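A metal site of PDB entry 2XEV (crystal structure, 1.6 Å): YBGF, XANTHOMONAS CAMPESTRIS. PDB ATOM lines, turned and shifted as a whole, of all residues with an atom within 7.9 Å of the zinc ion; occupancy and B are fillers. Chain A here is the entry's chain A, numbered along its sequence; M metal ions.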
ATOM      1  N   PHE A  55      21.484 -16.349   4.794  1.00  0.00           N
ATOM      2  CA  PHE A  55      22.038 -16.072   6.121  1.00  0.00           C
ATOM      3  C   PHE A  55      21.207 -16.581   7.291  1.00  0.00           C
ATOM      4  O   PHE A  55      21.777 -16.937   8.331  1.00  0.00           O
ATOM      5  CB  PHE A  55      22.311 -14.575   6.257  1.00  0.00           C
ATOM      6  CG  PHE A  55      23.279 -14.050   5.228  1.00  0.00           C
ATOM      7  CD1 PHE A  55      24.594 -14.502   5.189  1.00  0.00           C
ATOM      8  CD2 PHE A  55      22.857 -13.125   4.273  1.00  0.00           C
ATOM      9  CE1 PHE A  55      25.485 -14.028   4.238  1.00  0.00           C
ATOM     10  CE2 PHE A  55      23.751 -12.646   3.300  1.00  0.00           C
ATOM     11  CZ  PHE A  55      25.059 -13.094   3.280  1.00  0.00           C
ATOM     12  N   GLN A  56      19.882 -16.611   7.137  1.00  0.00           N
ATOM     13  CA  GLN A  56      19.026 -17.151   8.197  1.00  0.00           C
ATOM     14  C   GLN A  56      19.227 -18.631   8.335  1.00  0.00           C
ATOM     15  O   GLN A  56      19.308 -19.135   9.469  1.00  0.00           O
ATOM     16  CB  GLN A  56      17.547 -16.868   7.909  1.00  0.00           C
ATOM     17  CG  GLN A  56      17.263 -15.391   7.829  1.00  0.00           C
ATOM     18  CD  GLN A  56      17.114 -14.935   6.391  1.00  0.00           C
ATOM     19  OE1 GLN A  56      17.955 -15.211   5.523  1.00  0.00           O
ATOM     20  NE2 GLN A  56      16.014 -14.250   6.111  1.00  0.00           N
ATOM     21  N   GLU A  59      22.777 -19.127   9.858  1.00  0.00           N
ATOM     22  CA  GLU A  59      22.751 -18.800  11.280  1.00  0.00           C
ATOM     23  C   GLU A  59      22.319 -20.001  12.141  1.00  0.00           C
ATOM     24  O   GLU A  59      22.976 -20.302  13.138  1.00  0.00           O
ATOM     25  CB  GLU A  59      21.854 -17.590  11.506  1.00  0.00           C
ATOM     26  CG  GLU A  59      21.408 -17.372  12.912  1.00  0.00           C
ATOM     27  CD  GLU A  59      20.462 -16.184  12.976  1.00  0.00           C
ATOM     28  OE1 GLU A  59      19.323 -16.270  12.424  1.00  0.00           O
ATOM     29  OE2 GLU A  59      20.858 -15.163  13.562  1.00  0.00           O
ATOM     30  N   ALA A  60      21.244 -20.691  11.753  1.00  0.00           N
ATOM     31  CA  ALA A  60      20.787 -21.807  12.560  1.00  0.00           C
ATOM     32  C   ALA A  60      21.821 -22.919  12.716  1.00  0.00           C
ATOM     33  O   ALA A  60      21.940 -23.517  13.782  1.00  0.00           O
ATOM     34  CB  ALA A  60      19.454 -22.372  11.989  1.00  0.00           C
ATOM     35  N   ARG A  63      25.023 -21.590  14.828  1.00  0.00           N
ATOM     36  CA  ARG A  63      24.649 -21.409  16.242  1.00  0.00           C
ATOM     37  C   ARG A  63      24.599 -22.765  16.948  1.00  0.00           C
ATOM     38  O   ARG A  63      25.152 -22.928  18.058  1.00  0.00           O
ATOM     39  CB  ARG A  63      23.299 -20.688  16.374  1.00  0.00           C
ATOM     40  CG  ARG A  63      22.861 -20.504  17.809  1.00  0.00           C
ATOM     41  CD  ARG A  63      21.608 -19.640  17.886  1.00  0.00           C
ATOM     42  NE  ARG A  63      21.919 -18.219  17.706  1.00  0.00           N
ATOM     43  CZ  ARG A  63      21.185 -17.367  16.989  1.00  0.00           C
ATOM     44  NH1 ARG A  63      20.089 -17.771  16.355  1.00  0.00           N
ATOM     45  NH2 ARG A  63      21.549 -16.095  16.915  1.00  0.00           N
ATOM     46  N   LEU A  82      28.896 -17.549  12.271  1.00  0.00           N
ATOM     47  CA  LEU A  82      27.662 -17.093  12.902  1.00  0.00           C
ATOM     48  C   LEU A  82      27.574 -15.558  12.879  1.00  0.00           C
ATOM     49  O   LEU A  82      26.556 -14.994  12.454  1.00  0.00           O
ATOM     50  CB  LEU A  82      27.482 -17.620  14.337  1.00  0.00           C
ATOM     51  CG  LEU A  82      26.217 -17.096  15.053  1.00  0.00           C
ATOM     52  CD1 LEU A  82      24.926 -17.514  14.323  1.00  0.00           C
ATOM     53  CD2 LEU A  82      26.164 -17.567  16.511  1.00  0.00           C
ATOM     54  N   SER A  85      27.145 -14.277   9.386  1.00  0.00           N
ATOM     55  CA  SER A  85      25.762 -14.520   8.960  1.00  0.00           C
ATOM     56  C   SER A  85      24.787 -13.491   9.542  1.00  0.00           C
ATOM     57  O   SER A  85      23.854 -13.038   8.855  1.00  0.00           O
ATOM     58  CB  SER A  85      25.326 -15.953   9.334  1.00  0.00           C
ATOM     59  OG  SER A  85      26.100 -16.917   8.631  1.00  0.00           O
ATOM     60  N   GLN A  86      25.004 -13.107  10.802  1.00  0.00           N
ATOM     61  CA  GLN A  86      24.169 -12.104  11.457  1.00  0.00           C
ATOM     62  C   GLN A  86      24.354 -10.742  10.784  1.00  0.00           C
ATOM     63  O   GLN A  86      23.381 -10.017  10.552  1.00  0.00           O
ATOM     64  CB  GLN A  86      24.456 -12.080  12.948  1.00  0.00           C
ATOM     65  CG  GLN A  86      24.040 -13.392  13.598  1.00  0.00           C
ATOM     66  CD  GLN A  86      24.521 -13.550  15.014  1.00  0.00           C
ATOM     67  OE1 GLN A  86      25.545 -12.992  15.396  1.00  0.00           O
ATOM     68  NE2 GLN A  86      23.775 -14.325  15.807  1.00  0.00           N
ATOM     69  N   TYR A  87      25.599 -10.423  10.437  1.00  0.00           N
ATOM     70  CA  TYR A  87      25.874  -9.216   9.649  1.00  0.00           C
ATOM     71  C   TYR A  87      25.103  -9.266   8.319  1.00  0.00           C
ATOM     72  O   TYR A  87      24.492  -8.266   7.908  1.00  0.00           O
ATOM     73  CB  TYR A  87      27.377  -9.054   9.414  1.00  0.00           C
ATOM     74  CG  TYR A  87      27.766  -7.777   8.718  1.00  0.00           C
ATOM     75  CD1 TYR A  87      27.568  -6.541   9.336  1.00  0.00           C
ATOM     76  CD2 TYR A  87      28.337  -7.799   7.440  1.00  0.00           C
ATOM     77  CE1 TYR A  87      27.924  -5.349   8.696  1.00  0.00           C
ATOM     78  CE2 TYR A  87      28.696  -6.608   6.791  1.00  0.00           C
ATOM     79  CZ  TYR A  87      28.490  -5.391   7.430  1.00  0.00           C
ATOM     80  OH  TYR A  87      28.838  -4.218   6.812  1.00  0.00           O
ATOM     81  N   GLU A  89      22.321 -10.755   7.774  1.00  0.00           N
ATOM     82  CA  GLU A  89      20.914 -10.533   8.096  1.00  0.00           C
ATOM     83  C   GLU A  89      20.601  -9.059   8.349  1.00  0.00           C
ATOM     84  O   GLU A  89      19.434  -8.688   8.525  1.00  0.00           O
ATOM     85  CB  GLU A  89      20.521 -11.251   9.384  1.00  0.00           C
ATOM     86  CG  GLU A  89      20.344 -12.741   9.300  1.00  0.00           C
ATOM     87  CD  GLU A  89      19.819 -13.289  10.622  1.00  0.00           C
ATOM     88  OE1 GLU A  89      20.355 -12.910  11.712  1.00  0.00           O
ATOM     89  OE2 GLU A  89      18.828 -14.066  10.585  1.00  0.00           O
ATOM     90  N   GLY A  90      21.638  -8.238   8.436  1.00  0.00           N
ATOM     91  CA  GLY A  90      21.461  -6.833   8.767  1.00  0.00           C
ATOM     92  C   GLY A  90      21.316  -6.600  10.250  1.00  0.00           C
ATOM     93  O   GLY A  90      20.771  -5.577  10.668  1.00  0.00           O
ATOM     94  N   LYS A  91      21.794  -7.536  11.055  1.00  0.00           N
ATOM     95  CA  LYS A  91      21.716  -7.431  12.506  1.00  0.00           C
ATOM     96  C   LYS A  91      23.088  -7.043  13.065  1.00  0.00           C
ATOM     97  O   LYS A  91      23.810  -7.872  13.615  1.00  0.00           O
ATOM     98  CB  LYS A  91      21.230  -8.746  13.123  1.00  0.00           C
ATOM     99  CG  LYS A  91      19.874  -9.216  12.603  1.00  0.00           C
ATOM    100  CD  LYS A  91      18.736  -8.432  13.245  1.00  0.00           C
ATOM    101  CE  LYS A  91      17.418  -8.671  12.520  1.00  0.00           C
ATOM    102  NZ  LYS A  91      16.363  -7.734  13.005  1.00  0.00           N
ATOM    103  N   GLU A  94      24.048  -7.460  17.034  1.00  0.00           N
ATOM    104  CA  GLU A  94      24.243  -8.888  17.322  1.00  0.00           C
ATOM    105  C   GLU A  94      25.497  -9.483  16.645  1.00  0.00           C
ATOM    106  O   GLU A  94      26.239 -10.234  17.284  1.00  0.00           O
ATOM    107  CB  GLU A  94      22.921  -9.648  17.096  1.00  0.00           C
ATOM    108  CG  GLU A  94      22.867 -10.880  16.178  1.00  0.00           C
ATOM    109  CD  GLU A  94      21.438 -11.091  15.614  1.00  0.00           C
ATOM    110  OE1 GLU A  94      21.115 -12.187  15.096  1.00  0.00           O
ATOM    111  OE2 GLU A  94      20.633 -10.137  15.678  1.00  0.00           O
ATOM    112  N   ALA A  95      25.755  -9.107  15.390  1.00  0.00           N
ATOM    113  CA  ALA A  95      26.981  -9.500  14.681  1.00  0.00           C
ATOM    114  C   ALA A  95      28.273  -9.038  15.372  1.00  0.00           C
ATOM    115  O   ALA A  95      29.198  -9.830  15.514  1.00  0.00           O
ATOM    116  CB  ALA A  95      26.962  -8.991  13.257  1.00  0.00           C
HETATM  117 ZN    ZN M   1      20.117 -13.420  13.509  1.00  0.00          ZN
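O of Glu 94 sits close to OE1 of Gln 86 (3.4 Å).
The backbone carbonyl oxygen (O) of Gln 86 lies within hydrogen-bond range of the backbone NH (N) of Lys 91, 3.0 Å away.
The guanidinium group of Arg 63 sits close to the side-chain carboxylate of Glu 59, at 3.5 Å.
The side-chain amide nitrogen (NE2) of Gln 86 lies close to the guanidinium group (NH2) of Arg 63, 3.1 Å away.
Residues that only touch the zinc ion: Gln 86.
Four residues have an atom within 4 Å of the zinc ion: Glu 59, Gln 86, Glu 89 and Glu 94.
The zinc ion is bound by OE1 of Glu 89 (1.9 Å), OE2 of Glu 59 (1.9 Å) and OE1 of Glu 94 (2.2 Å).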
